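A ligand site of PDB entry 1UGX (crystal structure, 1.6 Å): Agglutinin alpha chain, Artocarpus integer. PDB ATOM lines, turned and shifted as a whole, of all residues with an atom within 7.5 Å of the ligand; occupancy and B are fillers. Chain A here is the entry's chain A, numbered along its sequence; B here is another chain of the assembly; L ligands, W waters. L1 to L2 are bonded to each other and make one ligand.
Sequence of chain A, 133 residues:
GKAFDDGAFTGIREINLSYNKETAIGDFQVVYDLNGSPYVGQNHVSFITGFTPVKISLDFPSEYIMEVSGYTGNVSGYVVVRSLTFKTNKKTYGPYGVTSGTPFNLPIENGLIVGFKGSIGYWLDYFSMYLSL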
ATOM      1  N   GLY A   1      17.878 -19.771  10.088  1.00  0.00           N
ATOM      2  CA  GLY A   1      18.125 -20.439   8.791  1.00  0.00           C
ATOM      3  C   GLY A   1      18.811 -21.780   8.956  1.00  0.00           C
ATOM      4  O   GLY A   1      19.093 -22.213  10.076  1.00  0.00           O
ATOM      5  N   LYS A   2      19.087 -22.442   7.834  1.00  0.00           N
ATOM      6  CA  LYS A   2      19.758 -23.738   7.865  1.00  0.00           C
ATOM      7  C   LYS A   2      21.258 -23.522   7.737  1.00  0.00           C
ATOM      8  O   LYS A   2      21.726 -23.017   6.721  1.00  0.00           O
ATOM      9  CB  LYS A   2      19.253 -24.608   6.714  1.00  0.00           C
ATOM     10  CG  LYS A   2      19.844 -26.010   6.706  1.00  0.00           C
ATOM     11  CD  LYS A   2      19.307 -26.805   5.520  1.00  0.00           C
ATOM     12  CE  LYS A   2      19.933 -28.182   5.445  1.00  0.00           C
ATOM     13  NZ  LYS A   2      19.405 -28.956   4.283  1.00  0.00           N
ATOM     14  N   ILE A  25      20.845 -11.440  -0.413  1.00  0.00           N
ATOM     15  CA  ILE A  25      21.436 -12.606  -1.064  1.00  0.00           C
ATOM     16  C   ILE A  25      20.611 -13.836  -0.734  1.00  0.00           C
ATOM     17  O   ILE A  25      20.151 -14.006   0.395  1.00  0.00           O
ATOM     18  CB  ILE A  25      22.890 -12.845  -0.574  1.00  0.00           C
ATOM     19  CG1 ILE A  25      23.761 -11.630  -0.922  1.00  0.00           C
ATOM     20  CG2 ILE A  25      23.445 -14.128  -1.195  1.00  0.00           C
ATOM     21  CD1 ILE A  25      23.787 -11.289  -2.391  1.00  0.00           C
ATOM     22  N   SER A  46      17.889 -20.929  -0.621  1.00  0.00           N
ATOM     23  CA  SER A  46      16.959 -20.144   0.189  1.00  0.00           C
ATOM     24  C   SER A  46      15.668 -20.949   0.345  1.00  0.00           C
ATOM     25  O   SER A  46      15.385 -21.840  -0.462  1.00  0.00           O
ATOM     26  CB  SER A  46      16.654 -18.820  -0.534  1.00  0.00           C
ATOM     27  OG  SER A  46      15.538 -18.173   0.047  1.00  0.00           O
ATOM     28  N   PHE A  47      14.912 -20.655   1.396  1.00  0.00           N
ATOM     29  CA  PHE A  47      13.644 -21.347   1.633  1.00  0.00           C
ATOM     30  C   PHE A  47      12.604 -20.826   0.637  1.00  0.00           C
ATOM     31  O   PHE A  47      11.572 -21.467   0.433  1.00  0.00           O
ATOM     32  CB  PHE A  47      13.112 -21.072   3.042  1.00  0.00           C
ATOM     33  CG  PHE A  47      13.997 -21.570   4.155  1.00  0.00           C
ATOM     34  CD1 PHE A  47      14.929 -22.579   3.934  1.00  0.00           C
ATOM     35  CD2 PHE A  47      13.844 -21.071   5.437  1.00  0.00           C
ATOM     36  CE1 PHE A  47      15.695 -23.074   4.983  1.00  0.00           C
ATOM     37  CE2 PHE A  47      14.612 -21.565   6.499  1.00  0.00           C
ATOM     38  CZ  PHE A  47      15.536 -22.567   6.265  1.00  0.00           C
ATOM     39  N   ILE A  48      12.884 -19.678   0.035  1.00  0.00           N
ATOM     40  CA  ILE A  48      11.951 -19.082  -0.921  1.00  0.00           C
ATOM     41  C   ILE A  48      12.569 -18.926  -2.306  1.00  0.00           C
ATOM     42  O   ILE A  48      13.725 -19.276  -2.519  1.00  0.00           O
ATOM     43  CB  ILE A  48      11.439 -17.705  -0.421  1.00  0.00           C
ATOM     44  CG1 ILE A  48      12.615 -16.776  -0.121  1.00  0.00           C
ATOM     45  CG2 ILE A  48      10.583 -17.906   0.827  1.00  0.00           C
ATOM     46  CD1 ILE A  48      12.207 -15.350   0.213  1.00  0.00           C
ATOM     47  N   VAL A  75      16.155  -7.032   7.075  1.00  0.00           N
ATOM     48  CA  VAL A  75      15.190  -7.316   6.022  1.00  0.00           C
ATOM     49  C   VAL A  75      14.080  -8.114   6.702  1.00  0.00           C
ATOM     50  O   VAL A  75      14.315  -9.211   7.211  1.00  0.00           O
ATOM     51  CB  VAL A  75      15.805  -8.167   4.880  1.00  0.00           C
ATOM     52  CG1 VAL A  75      14.732  -8.486   3.838  1.00  0.00           C
ATOM     53  CG2 VAL A  75      16.950  -7.403   4.229  1.00  0.00           C
ATOM     54  N   SER A  76      12.876  -7.542   6.735  1.00  0.00           N
ATOM     55  CA  SER A  76      11.741  -8.181   7.380  1.00  0.00           C
ATOM     56  C   SER A  76      12.029  -8.540   8.835  1.00  0.00           C
ATOM     57  O   SER A  76      11.514  -9.534   9.356  1.00  0.00           O
ATOM     58  CB  SER A  76      11.329  -9.433   6.602  1.00  0.00           C
ATOM     59  OG  SER A  76      10.872  -9.087   5.315  1.00  0.00           O
ATOM     60  N   GLY A  77      12.856  -7.733   9.486  1.00  0.00           N
ATOM     61  CA  GLY A  77      13.177  -7.964  10.887  1.00  0.00           C
ATOM     62  C   GLY A  77      14.373  -8.861  11.158  1.00  0.00           C
ATOM     63  O   GLY A  77      14.714  -9.090  12.319  1.00  0.00           O
ATOM     64  N   TYR A  78      15.016  -9.351  10.101  1.00  0.00           N
ATOM     65  CA  TYR A  78      16.177 -10.231  10.250  1.00  0.00           C
ATOM     66  C   TYR A  78      17.445  -9.580   9.731  1.00  0.00           C
ATOM     67  O   TYR A  78      17.430  -8.927   8.687  1.00  0.00           O
ATOM     68  CB  TYR A  78      15.973 -11.532   9.482  1.00  0.00           C
ATOM     69  CG  TYR A  78      14.797 -12.344   9.929  1.00  0.00           C
ATOM     70  CD1 TYR A  78      14.863 -13.105  11.091  1.00  0.00           C
ATOM     71  CD2 TYR A  78      13.616 -12.348   9.204  1.00  0.00           C
ATOM     72  CE1 TYR A  78      13.776 -13.859  11.524  1.00  0.00           C
ATOM     73  CE2 TYR A  78      12.521 -13.097   9.623  1.00  0.00           C
ATOM     74  CZ  TYR A  78      12.608 -13.853  10.775  1.00  0.00           C
ATOM     75  OH  TYR A  78      11.522 -14.595  11.177  1.00  0.00           O
ATOM     76  N   VAL A  79      18.543  -9.759  10.458  1.00  0.00           N
ATOM     77  CA  VAL A  79      19.814  -9.218  10.006  1.00  0.00           C
ATOM     78  C   VAL A  79      20.347 -10.256   9.011  1.00  0.00           C
ATOM     79  O   VAL A  79      20.465 -11.431   9.352  1.00  0.00           O
ATOM     80  CB  VAL A  79      20.812  -9.055  11.175  1.00  0.00           C
ATOM     81  CG1 VAL A  79      22.159  -8.559  10.663  1.00  0.00           C
ATOM     82  CG2 VAL A  79      20.239  -8.074  12.198  1.00  0.00           C
ATOM     83  N   VAL A  80      20.623  -9.815   7.791  1.00  0.00           N
ATOM     84  CA  VAL A  80      21.112 -10.711   6.744  1.00  0.00           C
ATOM     85  C   VAL A  80      22.184 -10.030   5.899  1.00  0.00           C
ATOM     86  O   VAL A  80      22.432  -8.844   6.030  1.00  0.00           O
ATOM     87  CB  VAL A  80      19.967 -11.161   5.803  1.00  0.00           C
ATOM     88  CG1 VAL A  80      18.907 -11.913   6.579  1.00  0.00           C
ATOM     89  CG2 VAL A  80      19.357  -9.940   5.114  1.00  0.00           C
ATOM     90  N   SER A 119      24.841 -19.681   7.004  1.00  0.00           N
ATOM     91  CA  SER A 119      23.461 -20.078   7.223  1.00  0.00           C
ATOM     92  C   SER A 119      22.555 -19.330   6.269  1.00  0.00           C
ATOM     93  O   SER A 119      22.747 -18.146   6.019  1.00  0.00           O
ATOM     94  CB  SER A 119      23.059 -19.773   8.654  1.00  0.00           C
ATOM     95  OG  SER A 119      21.663 -20.004   8.857  1.00  0.00           O
ATOM     96  N   ILE A 120      21.562 -20.035   5.724  1.00  0.00           N
ATOM     97  CA  ILE A 120      20.617 -19.419   4.817  1.00  0.00           C
ATOM     98  C   ILE A 120      19.203 -19.809   5.213  1.00  0.00           C
ATOM     99  O   ILE A 120      18.914 -20.984   5.438  1.00  0.00           O
ATOM    100  CB  ILE A 120      20.859 -19.869   3.349  1.00  0.00           C
ATOM    101  CG1 ILE A 120      22.288 -19.520   2.922  1.00  0.00           C
ATOM    102  CG2 ILE A 120      19.853 -19.201   2.406  1.00  0.00           C
ATOM    103  CD1 ILE A 120      22.644 -19.964   1.519  1.00  0.00           C
ATOM    104  N   GLY A 121      18.331 -18.810   5.319  1.00  0.00           N
ATOM    105  CA  GLY A 121      16.934 -19.048   5.638  1.00  0.00           C
ATOM    106  C   GLY A 121      16.234 -18.522   4.397  1.00  0.00           C
ATOM    107  O   GLY A 121      16.312 -19.134   3.343  1.00  0.00           O
ATOM    108  N   TYR A 122      15.553 -17.392   4.538  1.00  0.00           N
ATOM    109  CA  TYR A 122      14.927 -16.777   3.360  1.00  0.00           C
ATOM    110  C   TYR A 122      16.109 -16.142   2.631  1.00  0.00           C
ATOM    111  O   TYR A 122      16.166 -16.123   1.402  1.00  0.00           O
ATOM    112  CB  TYR A 122      13.930 -15.695   3.779  1.00  0.00           C
ATOM    113  CG  TYR A 122      12.530 -16.182   4.073  1.00  0.00           C
ATOM    114  CD1 TYR A 122      12.273 -17.537   4.293  1.00  0.00           C
ATOM    115  CD2 TYR A 122      11.462 -15.291   4.148  1.00  0.00           C
ATOM    116  CE1 TYR A 122      10.983 -17.986   4.589  1.00  0.00           C
ATOM    117  CE2 TYR A 122      10.170 -15.730   4.435  1.00  0.00           C
ATOM    118  CZ  TYR A 122       9.947 -17.083   4.651  1.00  0.00           C
ATOM    119  OH  TYR A 122       8.682 -17.524   4.964  1.00  0.00           O
ATOM    120  N   TRP A 123      17.069 -15.658   3.409  1.00  0.00           N
ATOM    121  CA  TRP A 123      18.256 -15.009   2.857  1.00  0.00           C
ATOM    122  C   TRP A 123      19.508 -15.516   3.565  1.00  0.00           C
ATOM    123  O   TRP A 123      19.414 -16.262   4.536  1.00  0.00           O
ATOM    124  CB  TRP A 123      18.146 -13.491   3.054  1.00  0.00           C
ATOM    125  CG  TRP A 123      16.896 -12.952   2.456  1.00  0.00           C
ATOM    126  CD1 TRP A 123      16.603 -12.861   1.124  1.00  0.00           C
ATOM    127  CD2 TRP A 123      15.708 -12.549   3.155  1.00  0.00           C
ATOM    128  NE1 TRP A 123      15.308 -12.425   0.944  1.00  0.00           N
ATOM    129  CE2 TRP A 123      14.733 -12.232   2.176  1.00  0.00           C
ATOM    130  CE3 TRP A 123      15.369 -12.429   4.513  1.00  0.00           C
ATOM    131  CZ2 TRP A 123      13.438 -11.808   2.510  1.00  0.00           C
ATOM    132  CZ3 TRP A 123      14.074 -12.005   4.847  1.00  0.00           C
ATOM    133  CH2 TRP A 123      13.132 -11.701   3.844  1.00  0.00           C
ATOM    134  N   LEU A 124      20.674 -15.101   3.066  1.00  0.00           N
ATOM    135  CA  LEU A 124      21.946 -15.481   3.665  1.00  0.00           C
ATOM    136  C   LEU A 124      22.023 -14.755   5.007  1.00  0.00           C
ATOM    137  O   LEU A 124      22.140 -13.525   5.047  1.00  0.00           O
ATOM    138  CB  LEU A 124      23.078 -15.052   2.743  1.00  0.00           C
ATOM    139  CG  LEU A 124      24.504 -15.340   3.222  1.00  0.00           C
ATOM    140  CD1 LEU A 124      24.703 -16.829   3.436  1.00  0.00           C
ATOM    141  CD2 LEU A 124      25.496 -14.810   2.202  1.00  0.00           C
ATOM    142  N   ASP A 125      21.939 -15.511   6.101  1.00  0.00           N
ATOM    143  CA  ASP A 125      21.956 -14.948   7.453  1.00  0.00           C
ATOM    144  C   ASP A 125      23.327 -14.423   7.835  1.00  0.00           C
ATOM    145  O   ASP A 125      23.471 -13.313   8.337  1.00  0.00           O
ATOM    146  CB  ASP A 125      21.534 -16.021   8.466  1.00  0.00           C
ATOM    147  CG  ASP A 125      20.166 -16.604   8.172  1.00  0.00           C
ATOM    148  OD1 ASP A 125      19.203 -15.820   8.034  1.00  0.00           O
ATOM    149  OD2 ASP A 125      20.059 -17.842   8.074  1.00  0.00           O
ATOM    150  N   TYR A 126      24.330 -15.258   7.601  1.00  0.00           N
ATOM    151  CA  TYR A 126      25.701 -14.904   7.915  1.00  0.00           C
ATOM    152  C   TYR A 126      26.630 -15.877   7.200  1.00  0.00           C
ATOM    153  O   TYR A 126      26.199 -16.923   6.709  1.00  0.00           O
ATOM    154  CB  TYR A 126      25.936 -14.968   9.431  1.00  0.00           C
ATOM    155  CG  TYR A 126      25.600 -16.300  10.076  1.00  0.00           C
ATOM    156  CD1 TYR A 126      26.466 -17.394   9.979  1.00  0.00           C
ATOM    157  CD2 TYR A 126      24.409 -16.466  10.792  1.00  0.00           C
ATOM    158  CE1 TYR A 126      26.140 -18.618  10.563  1.00  0.00           C
ATOM    159  CE2 TYR A 126      24.084 -17.677  11.381  1.00  0.00           C
ATOM    160  CZ  TYR A 126      24.952 -18.757  11.266  1.00  0.00           C
ATOM    161  OH  TYR A 126      24.620 -19.960  11.855  1.00  0.00           O
ATOM    162  N   GLY B  16      27.152 -10.737   9.431  1.00  0.00           N
ATOM    163  CA  GLY B  16      25.717 -10.903   9.276  1.00  0.00           C
ATOM    164  C   GLY B  16      25.073 -11.081  10.639  1.00  0.00           C
ATOM    165  O   GLY B  16      25.507 -10.434  11.602  1.00  0.00           O
ATOM    166  N   ALA B  17      24.057 -11.924  10.738  1.00  0.00           N
ATOM    167  CA  ALA B  17      23.380 -12.147  12.004  1.00  0.00           C
ATOM    168  C   ALA B  17      24.302 -12.814  13.022  1.00  0.00           C
ATOM    169  O   ALA B  17      25.174 -13.596  12.652  1.00  0.00           O
ATOM    170  CB  ALA B  17      22.149 -13.001  11.800  1.00  0.00           C
ATOM    171  N   LYS B  18      24.124 -12.503  14.302  1.00  0.00           N
ATOM    172  CA  LYS B  18      24.964 -13.108  15.336  1.00  0.00           C
ATOM    173  C   LYS B  18      24.217 -14.228  16.042  1.00  0.00           C
ATOM    174  O   LYS B  18      24.595 -15.411  15.883  1.00  0.00           O
ATOM    175  CB  LYS B  18      25.403 -12.041  16.334  1.00  0.00           C
ATOM    176  CG  LYS B  18      26.541 -11.159  15.846  1.00  0.00           C
ATOM    177  CD  LYS B  18      27.166 -10.399  16.983  1.00  0.00           C
ATOM    178  CE  LYS B  18      28.349  -9.582  16.507  1.00  0.00           C
ATOM    179  NZ  LYS B  18      29.054  -8.963  17.657  1.00  0.00           N
HETATM  180  O1  LIG L   1      17.027 -15.538   6.294  1.00  0.00           O
HETATM  181  C1  LIG L   1      16.262 -14.769   7.201  1.00  0.00           C
HETATM  182  C2  LIG L   1      15.380 -15.613   8.134  1.00  0.00           C
HETATM  183  O2  LIG L   1      14.609 -16.678   7.365  1.00  0.00           O
HETATM  184  C3  LIG L   1      13.691 -17.560   8.143  1.00  0.00           C
HETATM  185  O3  LIG L   1      12.602 -16.767   8.639  1.00  0.00           O
HETATM  186  C4  LIG L   1      11.655 -16.003   7.644  1.00  0.00           C
HETATM  187  C5  LIG L   1      14.482 -18.224   9.271  1.00  0.00           C
HETATM  188  N1  LIG L   1      13.505 -19.020   9.906  1.00  0.00           N
HETATM  189  C6  LIG L   1      13.703 -20.306  10.319  1.00  0.00           C
HETATM  190  O4  LIG L   1      14.603 -21.044   9.873  1.00  0.00           O
HETATM  191  C7  LIG L   1      12.765 -20.854  11.386  1.00  0.00           C
HETATM  192  C8  LIG L   1      15.171 -17.157  10.130  1.00  0.00           C
HETATM  193  O5  LIG L   1      15.855 -17.810  11.155  1.00  0.00           O
HETATM  194  C9  LIG L   1      16.217 -16.356   9.269  1.00  0.00           C
HETATM  195  O6  LIG L   1      17.132 -17.332   8.715  1.00  0.00           O
HETATM  196  C1  LG2 L   2      15.990 -17.434  12.536  1.00  0.00           C
HETATM  197  C2  LG2 L   2      16.291 -18.527  13.540  1.00  0.00           C
HETATM  198  C3  LG2 L   2      16.665 -17.907  14.883  1.00  0.00           C
HETATM  199  C4  LG2 L   2      17.980 -16.992  14.735  1.00  0.00           C
HETATM  200  C5  LG2 L   2      17.668 -15.858  13.704  1.00  0.00           C
HETATM  201  C6  LG2 L   2      18.540 -14.727  13.204  1.00  0.00           C
HETATM  202  O1  LG2 L   2      15.130 -19.347  13.618  1.00  0.00           O
HETATM  203  O2  LG2 L   2      16.943 -18.959  15.818  1.00  0.00           O
HETATM  204  O3  LG2 L   2      19.087 -17.746  14.216  1.00  0.00           O
HETATM  205  O4  LG2 L   2      17.174 -16.520  12.412  1.00  0.00           O
HETATM  206  O5  LG2 L   2      18.392 -13.647  12.290  1.00  0.00           O
HETATM  207  O   HOH W   1      18.975 -13.720   9.806  1.00  0.00           O
HETATM  208  O   HOH W   2      15.892 -23.629  10.148  1.00  0.00           O
HETATM  209  O   HOH W   3      11.444 -17.560  11.589  1.00  0.00           O
HETATM  210  O   HOH W   4      16.538 -21.541  12.433  1.00  0.00           O
HETATM  211  O   HOH W   5      18.689 -11.210  13.145  1.00  0.00           O
HETATM  212  O   HOH W   6      12.549 -17.644  13.987  1.00  0.00           O
HETATM  213  O   HOH W   7      20.015 -19.054  11.606  1.00  0.00           O
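O6 of LIG L1 sits at hydrogen-bond distance from OD1 of Asp 125, at 2.7 Å. The backbone NH of Trp 123 lies within hydrogen-bond range of an oxygen (O1) of LIG L1, at 2.9 Å. The backbone carbonyl oxygen of Trp 123 is in hydrogen-bond range of an oxygen (O1) of LIG L1 (3.1 Å). An oxygen (O6) of LIG L1 sits at hydrogen-bond distance from the backbone NH (N) of Gly 1. The backbone NH (N) of Tyr 122 sits at hydrogen-bond distance from an oxygen (O1) of LIG L1 (2.9 Å).
The side-chain carboxylate of Asp 125 sits at hydrogen-bond distance from the backbone NH of Gly 121, 3.4 Å away. The backbone carbonyl oxygen (O) of Asp 125 sits at hydrogen-bond distance from the backbone NH (N) of Ala 17 of chain B (2.8 Å). N of Asp 125 is in hydrogen-bond range of O of Ser 119 (2.8 Å). The backbone carbonyl oxygen (O) of Tyr 122 sits at hydrogen-bond distance from the side-chain hydroxyl (OG) of Ser 46, 2.5 Å away. The backbone NH of Phe 47 sits at hydrogen-bond distance from the backbone carbonyl oxygen of Gly 121.
Residues that only touch the ligand: Phe 47 (3.4 Å), Tyr 78 (3.5 Å), Gly 121 (3.5 Å), Ala 17 of chain B (3.8 Å) and Val 80 (3.9 Å). Hydrophobic or aromatic side chains within 4 Å of the ligand: Phe 47, Tyr 78, Val 80, Tyr 122, Trp 123 and Ala 17 of chain B. Nine residues have an atom within 4 Å of the ligand: Gly 1, Phe 47, Tyr 78, Val 80, Gly 121, Tyr 122, Trp 123, Asp 125 and Ala 17 of chain B. Along chain A the residues within 4 Å of the ligand span positions 1 to 125. The nearest printed residue that does not touch the ligand is Val 79 (4.2 Å).
Water W1 lies within hydrogen-bond range of O5 of LG2 L2 (2.6 Å), OD1 of Asp 125 (2.8 Å) and O of Val 79 (2.8 Å). Water W5 bridges an oxygen (O5) of LG2 L2 and the backbone NH of Val 79. Water W4 lies within hydrogen-bond range of O1 of LG2 L2 and N of Gly 1. Water W3 lies within hydrogen-bond range of the side-chain hydroxyl (OH) of Tyr 78 (3.0 Å) and a nitrogen (N1) of LIG L1 (3.0 Å). Water W7 lies within hydrogen-bond range of N of Gly 1, O3 of LG2 L2 and OG of Ser 119.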
